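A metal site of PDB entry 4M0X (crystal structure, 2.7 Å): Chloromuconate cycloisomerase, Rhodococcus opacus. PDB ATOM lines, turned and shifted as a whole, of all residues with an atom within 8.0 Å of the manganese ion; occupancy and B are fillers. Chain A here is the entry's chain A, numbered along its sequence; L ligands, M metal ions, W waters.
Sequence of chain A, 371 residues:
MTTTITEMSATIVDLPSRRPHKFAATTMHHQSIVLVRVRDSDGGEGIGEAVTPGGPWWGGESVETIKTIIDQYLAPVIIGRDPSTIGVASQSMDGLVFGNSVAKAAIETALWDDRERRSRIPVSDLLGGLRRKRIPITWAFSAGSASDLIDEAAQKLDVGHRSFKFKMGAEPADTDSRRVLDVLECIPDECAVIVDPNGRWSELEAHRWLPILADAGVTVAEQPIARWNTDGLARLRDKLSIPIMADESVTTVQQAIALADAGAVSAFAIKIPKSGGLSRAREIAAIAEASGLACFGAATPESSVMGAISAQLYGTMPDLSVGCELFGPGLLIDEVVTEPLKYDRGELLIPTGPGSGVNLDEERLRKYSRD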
ATOM      1  N   PHE A  23      29.581 -24.312  -4.323  1.00  0.00           N
ATOM      2  CA  PHE A  23      29.630 -23.073  -3.548  1.00  0.00           C
ATOM      3  C   PHE A  23      29.462 -21.897  -4.499  1.00  0.00           C
ATOM      4  O   PHE A  23      29.123 -22.080  -5.671  1.00  0.00           O
ATOM      5  CB  PHE A  23      30.976 -22.935  -2.831  1.00  0.00           C
ATOM      6  CG  PHE A  23      31.275 -24.034  -1.830  1.00  0.00           C
ATOM      7  CD1 PHE A  23      30.836 -23.929  -0.508  1.00  0.00           C
ATOM      8  CD2 PHE A  23      32.005 -25.162  -2.207  1.00  0.00           C
ATOM      9  CE1 PHE A  23      31.113 -24.946   0.405  1.00  0.00           C
ATOM     10  CE2 PHE A  23      32.278 -26.168  -1.302  1.00  0.00           C
ATOM     11  CZ  PHE A  23      31.834 -26.065   0.007  1.00  0.00           C
ATOM     12  N   TRP A  57      39.434 -19.565  -3.420  1.00  0.00           N
ATOM     13  CA  TRP A  57      38.359 -18.581  -3.591  1.00  0.00           C
ATOM     14  C   TRP A  57      37.880 -17.992  -2.250  1.00  0.00           C
ATOM     15  O   TRP A  57      37.617 -16.800  -2.158  1.00  0.00           O
ATOM     16  CB  TRP A  57      37.183 -19.190  -4.380  1.00  0.00           C
ATOM     17  CG  TRP A  57      36.314 -20.122  -3.541  1.00  0.00           C
ATOM     18  CD1 TRP A  57      36.493 -21.462  -3.353  1.00  0.00           C
ATOM     19  CD2 TRP A  57      35.166 -19.755  -2.754  1.00  0.00           C
ATOM     20  NE1 TRP A  57      35.522 -21.965  -2.513  1.00  0.00           N
ATOM     21  CE2 TRP A  57      34.689 -20.943  -2.124  1.00  0.00           C
ATOM     22  CE3 TRP A  57      34.486 -18.544  -2.503  1.00  0.00           C
ATOM     23  CZ2 TRP A  57      33.576 -20.950  -1.262  1.00  0.00           C
ATOM     24  CZ3 TRP A  57      33.373 -18.559  -1.665  1.00  0.00           C
ATOM     25  CH2 TRP A  57      32.932 -19.759  -1.051  1.00  0.00           C
ATOM     26  N   TRP A  58      37.816 -18.828  -1.202  1.00  0.00           N
ATOM     27  CA  TRP A  58      37.237 -18.412   0.070  1.00  0.00           C
ATOM     28  C   TRP A  58      38.222 -17.630   0.919  1.00  0.00           C
ATOM     29  O   TRP A  58      37.901 -16.555   1.411  1.00  0.00           O
ATOM     30  CB  TRP A  58      36.752 -19.647   0.823  1.00  0.00           C
ATOM     31  CG  TRP A  58      35.841 -19.423   2.046  1.00  0.00           C
ATOM     32  CD1 TRP A  58      34.503 -19.690   2.121  1.00  0.00           C
ATOM     33  CD2 TRP A  58      36.232 -18.955   3.360  1.00  0.00           C
ATOM     34  NE1 TRP A  58      34.033 -19.408   3.379  1.00  0.00           N
ATOM     35  CE2 TRP A  58      35.061 -18.937   4.152  1.00  0.00           C
ATOM     36  CE3 TRP A  58      37.450 -18.530   3.927  1.00  0.00           C
ATOM     37  CZ2 TRP A  58      35.076 -18.511   5.490  1.00  0.00           C
ATOM     38  CZ3 TRP A  58      37.459 -18.097   5.277  1.00  0.00           C
ATOM     39  CH2 TRP A  58      36.282 -18.090   6.033  1.00  0.00           C
ATOM     40  N   LYS A 165      20.634 -25.635   5.949  1.00  0.00           N
ATOM     41  CA  LYS A 165      21.377 -24.536   5.362  1.00  0.00           C
ATOM     42  C   LYS A 165      21.269 -24.656   3.876  1.00  0.00           C
ATOM     43  O   LYS A 165      21.410 -25.754   3.328  1.00  0.00           O
ATOM     44  CB  LYS A 165      22.852 -24.603   5.775  1.00  0.00           C
ATOM     45  CG  LYS A 165      23.636 -23.336   5.529  1.00  0.00           C
ATOM     46  CD  LYS A 165      25.008 -23.496   6.170  1.00  0.00           C
ATOM     47  CE  LYS A 165      25.984 -22.453   5.670  1.00  0.00           C
ATOM     48  NZ  LYS A 165      27.385 -22.909   5.855  1.00  0.00           N
ATOM     49  N   LYS A 167      23.089 -23.378   0.518  1.00  0.00           N
ATOM     50  CA  LYS A 167      24.314 -22.755   0.052  1.00  0.00           C
ATOM     51  C   LYS A 167      23.857 -21.883  -1.109  1.00  0.00           C
ATOM     52  O   LYS A 167      23.008 -22.310  -1.884  1.00  0.00           O
ATOM     53  CB  LYS A 167      25.363 -23.806  -0.341  1.00  0.00           C
ATOM     54  CG  LYS A 167      26.769 -23.483   0.143  1.00  0.00           C
ATOM     55  CD  LYS A 167      27.176 -24.260   1.404  1.00  0.00           C
ATOM     56  CE  LYS A 167      27.915 -23.393   2.457  1.00  0.00           C
ATOM     57  NZ  LYS A 167      28.629 -22.154   1.987  1.00  0.00           N
ATOM     58  N   ILE A 194      19.293 -21.602   7.704  1.00  0.00           N
ATOM     59  CA  ILE A 194      20.290 -20.599   7.399  1.00  0.00           C
ATOM     60  C   ILE A 194      20.376 -20.456   5.889  1.00  0.00           C
ATOM     61  O   ILE A 194      20.256 -21.446   5.188  1.00  0.00           O
ATOM     62  CB  ILE A 194      21.672 -21.051   7.866  1.00  0.00           C
ATOM     63  CG1 ILE A 194      21.717 -21.166   9.369  1.00  0.00           C
ATOM     64  CG2 ILE A 194      22.779 -20.125   7.330  1.00  0.00           C
ATOM     65  CD1 ILE A 194      22.764 -22.144   9.843  1.00  0.00           C
ATOM     66  N   VAL A 195      20.605 -19.243   5.393  1.00  0.00           N
ATOM     67  CA  VAL A 195      21.079 -19.060   3.988  1.00  0.00           C
ATOM     68  C   VAL A 195      22.476 -18.416   3.934  1.00  0.00           C
ATOM     69  O   VAL A 195      22.744 -17.425   4.645  1.00  0.00           O
ATOM     70  CB  VAL A 195      20.085 -18.257   3.117  1.00  0.00           C
ATOM     71  CG1 VAL A 195      18.731 -18.967   3.077  1.00  0.00           C
ATOM     72  CG2 VAL A 195      19.921 -16.854   3.627  1.00  0.00           C
ATOM     73  N   ASP A 196      23.351 -18.989   3.116  1.00  0.00           N
ATOM     74  CA  ASP A 196      24.751 -18.558   3.026  1.00  0.00           C
ATOM     75  C   ASP A 196      25.223 -18.177   1.611  1.00  0.00           C
ATOM     76  O   ASP A 196      25.699 -19.033   0.864  1.00  0.00           O
ATOM     77  CB  ASP A 196      25.677 -19.627   3.576  1.00  0.00           C
ATOM     78  CG  ASP A 196      27.073 -19.108   3.805  1.00  0.00           C
ATOM     79  OD1 ASP A 196      27.284 -17.930   3.476  1.00  0.00           O
ATOM     80  OD2 ASP A 196      27.944 -19.853   4.306  1.00  0.00           O
ATOM     81  N   PRO A 197      25.079 -16.892   1.235  1.00  0.00           N
ATOM     82  CA  PRO A 197      25.556 -16.369  -0.033  1.00  0.00           C
ATOM     83  C   PRO A 197      27.072 -16.213  -0.089  1.00  0.00           C
ATOM     84  O   PRO A 197      27.598 -15.762  -1.092  1.00  0.00           O
ATOM     85  CB  PRO A 197      24.919 -14.981  -0.094  1.00  0.00           C
ATOM     86  CG  PRO A 197      23.816 -15.002   0.892  1.00  0.00           C
ATOM     87  CD  PRO A 197      24.272 -15.908   1.969  1.00  0.00           C
ATOM     88  N   ASN A 198      27.788 -16.530   0.972  1.00  0.00           N
ATOM     89  CA  ASN A 198      29.237 -16.460   0.930  1.00  0.00           C
ATOM     90  C   ASN A 198      29.732 -15.061   0.648  1.00  0.00           C
ATOM     91  O   ASN A 198      30.728 -14.857  -0.036  1.00  0.00           O
ATOM     92  CB  ASN A 198      29.777 -17.456  -0.097  1.00  0.00           C
ATOM     93  CG  ASN A 198      29.650 -18.897   0.369  1.00  0.00           C
ATOM     94  OD1 ASN A 198      30.345 -19.309   1.294  1.00  0.00           O
ATOM     95  ND2 ASN A 198      28.741 -19.683  -0.253  1.00  0.00           N
ATOM     96  N   GLY A 199      28.993 -14.088   1.171  1.00  0.00           N
ATOM     97  CA  GLY A 199      29.363 -12.682   1.065  1.00  0.00           C
ATOM     98  C   GLY A 199      29.310 -12.113  -0.336  1.00  0.00           C
ATOM     99  O   GLY A 199      29.907 -11.087  -0.604  1.00  0.00           O
ATOM    100  N   GLU A 222      23.616 -16.071   6.920  1.00  0.00           N
ATOM    101  CA  GLU A 222      25.031 -16.167   7.080  1.00  0.00           C
ATOM    102  C   GLU A 222      25.684 -15.260   6.060  1.00  0.00           C
ATOM    103  O   GLU A 222      25.209 -15.145   4.942  1.00  0.00           O
ATOM    104  CB  GLU A 222      25.496 -17.617   6.918  1.00  0.00           C
ATOM    105  CG  GLU A 222      26.831 -17.852   7.604  1.00  0.00           C
ATOM    106  CD  GLU A 222      27.492 -19.177   7.275  1.00  0.00           C
ATOM    107  OE1 GLU A 222      26.738 -20.181   7.124  1.00  0.00           O
ATOM    108  OE2 GLU A 222      28.741 -19.205   7.206  1.00  0.00           O
ATOM    109  N   GLN A 223      26.763 -14.588   6.465  1.00  0.00           N
ATOM    110  CA  GLN A 223      27.560 -13.719   5.625  1.00  0.00           C
ATOM    111  C   GLN A 223      26.870 -13.318   4.338  1.00  0.00           C
ATOM    112  O   GLN A 223      27.212 -13.830   3.275  1.00  0.00           O
ATOM    113  CB  GLN A 223      28.876 -14.393   5.266  1.00  0.00           C
ATOM    114  CG  GLN A 223      29.912 -13.405   4.742  1.00  0.00           C
ATOM    115  CD  GLN A 223      30.359 -12.477   5.835  1.00  0.00           C
ATOM    116  OE1 GLN A 223      30.743 -12.928   6.926  1.00  0.00           O
ATOM    117  NE2 GLN A 223      30.311 -11.178   5.568  1.00  0.00           N
ATOM    118  N   MET A 245      24.677 -13.806  10.809  1.00  0.00           N
ATOM    119  CA  MET A 245      25.880 -14.463  11.277  1.00  0.00           C
ATOM    120  C   MET A 245      27.133 -14.118  10.465  1.00  0.00           C
ATOM    121  O   MET A 245      27.147 -14.222   9.243  1.00  0.00           O
ATOM    122  CB  MET A 245      25.639 -15.946  11.231  1.00  0.00           C
ATOM    123  CG  MET A 245      26.814 -16.832  11.577  1.00  0.00           C
ATOM    124  SD  MET A 245      26.150 -18.399  12.179  1.00  0.00           S
ATOM    125  CE  MET A 245      25.326 -19.094  10.753  1.00  0.00           C
ATOM    126  N   ALA A 246      28.191 -13.747  11.164  1.00  0.00           N
ATOM    127  CA  ALA A 246      29.475 -13.568  10.566  1.00  0.00           C
ATOM    128  C   ALA A 246      30.151 -14.922  10.402  1.00  0.00           C
ATOM    129  O   ALA A 246      30.114 -15.777  11.302  1.00  0.00           O
ATOM    130  CB  ALA A 246      30.323 -12.684  11.457  1.00  0.00           C
ATOM    131  N   ASP A 247      30.762 -15.127   9.237  1.00  0.00           N
ATOM    132  CA  ASP A 247      31.571 -16.289   8.984  1.00  0.00           C
ATOM    133  C   ASP A 247      32.913 -15.733   8.482  1.00  0.00           C
ATOM    134  O   ASP A 247      33.812 -15.482   9.304  1.00  0.00           O
ATOM    135  CB  ASP A 247      30.915 -17.245   7.988  1.00  0.00           C
ATOM    136  CG  ASP A 247      31.841 -18.393   7.552  1.00  0.00           C
ATOM    137  OD1 ASP A 247      32.937 -18.542   8.159  1.00  0.00           O
ATOM    138  OD2 ASP A 247      31.497 -19.134   6.597  1.00  0.00           O
ATOM    139  N   GLU A 248      33.026 -15.500   7.162  1.00  0.00           N
ATOM    140  CA  GLU A 248      34.217 -14.874   6.551  1.00  0.00           C
ATOM    141  C   GLU A 248      34.694 -13.621   7.294  1.00  0.00           C
ATOM    142  O   GLU A 248      35.865 -13.272   7.206  1.00  0.00           O
ATOM    143  CB  GLU A 248      33.921 -14.447   5.112  1.00  0.00           C
ATOM    144  CG  GLU A 248      33.863 -15.530   4.039  1.00  0.00           C
ATOM    145  CD  GLU A 248      32.479 -16.144   3.945  1.00  0.00           C
ATOM    146  OE1 GLU A 248      31.676 -16.052   4.921  1.00  0.00           O
ATOM    147  OE2 GLU A 248      32.205 -16.735   2.876  1.00  0.00           O
ATOM    148  N   ALA A 269      30.073 -17.816  13.253  1.00  0.00           N
ATOM    149  CA  ALA A 269      30.279 -19.182  12.804  1.00  0.00           C
ATOM    150  C   ALA A 269      31.682 -19.543  13.280  1.00  0.00           C
ATOM    151  O   ALA A 269      32.649 -18.933  12.861  1.00  0.00           O
ATOM    152  CB  ALA A 269      30.180 -19.260  11.300  1.00  0.00           C
ATOM    153  N   LYS A 271      34.937 -22.028  13.568  1.00  0.00           N
ATOM    154  CA  LYS A 271      35.595 -23.016  12.695  1.00  0.00           C
ATOM    155  C   LYS A 271      37.061 -22.930  12.980  1.00  0.00           C
ATOM    156  O   LYS A 271      37.576 -21.834  13.010  1.00  0.00           O
ATOM    157  CB  LYS A 271      35.433 -22.648  11.227  1.00  0.00           C
ATOM    158  CG  LYS A 271      34.098 -22.869  10.563  1.00  0.00           C
ATOM    159  CD  LYS A 271      34.271 -22.896   9.046  1.00  0.00           C
ATOM    160  CE  LYS A 271      33.969 -21.562   8.385  1.00  0.00           C
ATOM    161  NZ  LYS A 271      32.675 -21.587   7.657  1.00  0.00           N
ATOM    162  N   LYS A 274      39.960 -21.669   9.690  1.00  0.00           N
ATOM    163  CA  LYS A 274      39.883 -20.255   9.405  1.00  0.00           C
ATOM    164  C   LYS A 274      40.426 -19.323  10.520  1.00  0.00           C
ATOM    165  O   LYS A 274      40.765 -18.174  10.241  1.00  0.00           O
ATOM    166  CB  LYS A 274      38.442 -19.955   8.958  1.00  0.00           C
ATOM    167  CG  LYS A 274      37.725 -18.786   9.571  1.00  0.00           C
ATOM    168  CD  LYS A 274      36.499 -19.225  10.342  1.00  0.00           C
ATOM    169  CE  LYS A 274      35.474 -18.107  10.240  1.00  0.00           C
ATOM    170  NZ  LYS A 274      34.319 -18.172  11.172  1.00  0.00           N
ATOM    171  N   PHE A 296      27.782 -20.854  16.248  1.00  0.00           N
ATOM    172  CA  PHE A 296      27.408 -21.875  15.347  1.00  0.00           C
ATOM    173  C   PHE A 296      28.643 -22.713  15.221  1.00  0.00           C
ATOM    174  O   PHE A 296      29.754 -22.170  15.089  1.00  0.00           O
ATOM    175  CB  PHE A 296      27.105 -21.247  14.004  1.00  0.00           C
ATOM    176  CG  PHE A 296      26.579 -22.208  12.981  1.00  0.00           C
ATOM    177  CD1 PHE A 296      25.514 -23.073  13.278  1.00  0.00           C
ATOM    178  CD2 PHE A 296      27.079 -22.177  11.688  1.00  0.00           C
ATOM    179  CE1 PHE A 296      24.992 -23.910  12.300  1.00  0.00           C
ATOM    180  CE2 PHE A 296      26.559 -23.012  10.701  1.00  0.00           C
ATOM    181  CZ  PHE A 296      25.519 -23.889  11.011  1.00  0.00           C
ATOM    182  N   ALA A 298      30.530 -24.384  12.984  1.00  0.00           N
ATOM    183  CA  ALA A 298      30.574 -24.275  11.540  1.00  0.00           C
ATOM    184  C   ALA A 298      31.501 -25.272  10.882  1.00  0.00           C
ATOM    185  O   ALA A 298      32.402 -25.825  11.526  1.00  0.00           O
ATOM    186  CB  ALA A 298      30.917 -22.869  11.111  1.00  0.00           C
ATOM    187  N   ALA A 299      31.298 -25.475   9.586  1.00  0.00           N
ATOM    188  CA  ALA A 299      32.045 -26.451   8.810  1.00  0.00           C
ATOM    189  C   ALA A 299      32.844 -25.741   7.725  1.00  0.00           C
ATOM    190  O   ALA A 299      32.468 -24.637   7.303  1.00  0.00           O
ATOM    191  CB  ALA A 299      31.089 -27.450   8.193  1.00  0.00           C
ATOM    192  N   THR A 300      33.928 -26.359   7.279  1.00  0.00           N
ATOM    193  CA  THR A 300      34.771 -25.770   6.244  1.00  0.00           C
ATOM    194  C   THR A 300      34.360 -26.162   4.810  1.00  0.00           C
ATOM    195  O   THR A 300      34.345 -25.325   3.914  1.00  0.00           O
ATOM    196  CB  THR A 300      36.278 -25.966   6.555  1.00  0.00           C
ATOM    197  OG1 THR A 300      36.611 -25.219   7.732  1.00  0.00           O
ATOM    198  CG2 THR A 300      37.118 -25.446   5.427  1.00  0.00           C
ATOM    199  N   GLU A 325      27.044 -27.556  11.969  1.00  0.00           N
ATOM    200  CA  GLU A 325      26.962 -28.077  10.622  1.00  0.00           C
ATOM    201  C   GLU A 325      28.070 -29.095  10.314  1.00  0.00           C
ATOM    202  O   GLU A 325      28.621 -29.090   9.215  1.00  0.00           O
ATOM    203  CB  GLU A 325      26.979 -26.921   9.578  1.00  0.00           C
ATOM    204  CG  GLU A 325      28.180 -25.976   9.713  1.00  0.00           C
ATOM    205  CD  GLU A 325      28.356 -25.002   8.547  1.00  0.00           C
ATOM    206  OE1 GLU A 325      27.514 -24.960   7.606  1.00  0.00           O
ATOM    207  OE2 GLU A 325      29.358 -24.263   8.541  1.00  0.00           O
HETATM  208 CL1  LIG L   1      31.018 -21.997   4.351  1.00  0.00          CL
HETATM  209 MN    MN M   1      29.746 -19.784   5.398  1.00  0.00          MN
HETATM  210  O   HOH W   1      29.691 -17.662   4.731  1.00  0.00           O
HETATM  211  O   HOH W   2      29.843 -21.722   7.279  1.00  0.00           O
HETATM  212  O   HOH W   3      31.346 -19.549   3.496  1.00  0.00           O
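The side-chain amino group (NZ) of Lys 165 sits close to the side-chain carboxylate (OD2) of Asp 196, at 3.5 Å.
The side-chain carboxylate (OD1) of Asp 196 sits at hydrogen-bond distance from the backbone NH (N) of Asn 198, at 2.9 Å.
The side-chain carboxylate (OD2) of Asp 196 sits close to the side-chain amino group (NZ) of Lys 167 (3.3 Å).
The side-chain carboxylate of Glu 222 is in salt-bridge range of the side-chain amino group of Lys 165 (3.1 Å).
O of Val 195 sits at hydrogen-bond distance from N of Glu 222.
The side-chain carboxylate (OD1) of Asp 247 lies within salt-bridge range of the side-chain amino group (NZ) of Lys 271 (3.1 Å).
OD1 of Asp 247 is in salt-bridge range of NZ of Lys 274.
NZ of Lys 165 lies within salt-bridge range of OE1 of Glu 325 (2.7 Å).
Residues that only touch the manganese ion: Lys 165.
Within 4 Å of the manganese ion: Lys 165, Asp 196, Glu 222 and Asp 247.
The nearest printed residue that does not touch the manganese ion is Lys 271 (4.1 Å).
OD2 of Asp 196 binds the manganese ion, 2.1 Å away.
OE2 of Glu 222 binds the manganese ion (2.1 Å).
The manganese ion is bound by the side-chain carboxylate (OD2) of Asp 247, 2.2 Å away.
The manganese ion is bound by water W1 (2.2 Å).
Water W3 binds the manganese ion, at 2.5 Å.
The manganese ion is bound by CL1 of the ligand, 2.8 Å away.
The manganese ion has six donor atoms within binding distance.
Slightly farther from the manganese ion lies water W2 (2.7 Å).
Water W1 bridges OE1 of Glu 248 (2.6 Å) and OD1 of Asp 196 (2.7 Å).
Water W3 lies within hydrogen-bond range of OD1 of Asn 198, NE1 of Trp 58 and OE2 of Glu 248.
Water W2 lies within hydrogen-bond range of the side-chain amino group (NZ) of Lys 271 (2.9 Å), the side-chain carboxylate (OE2) of Glu 325 (2.9 Å), the side-chain amino group (NZ) of Lys 165 (3.1 Å) and the side-chain carboxylate (OE1) of Glu 222 (3.5 Å).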
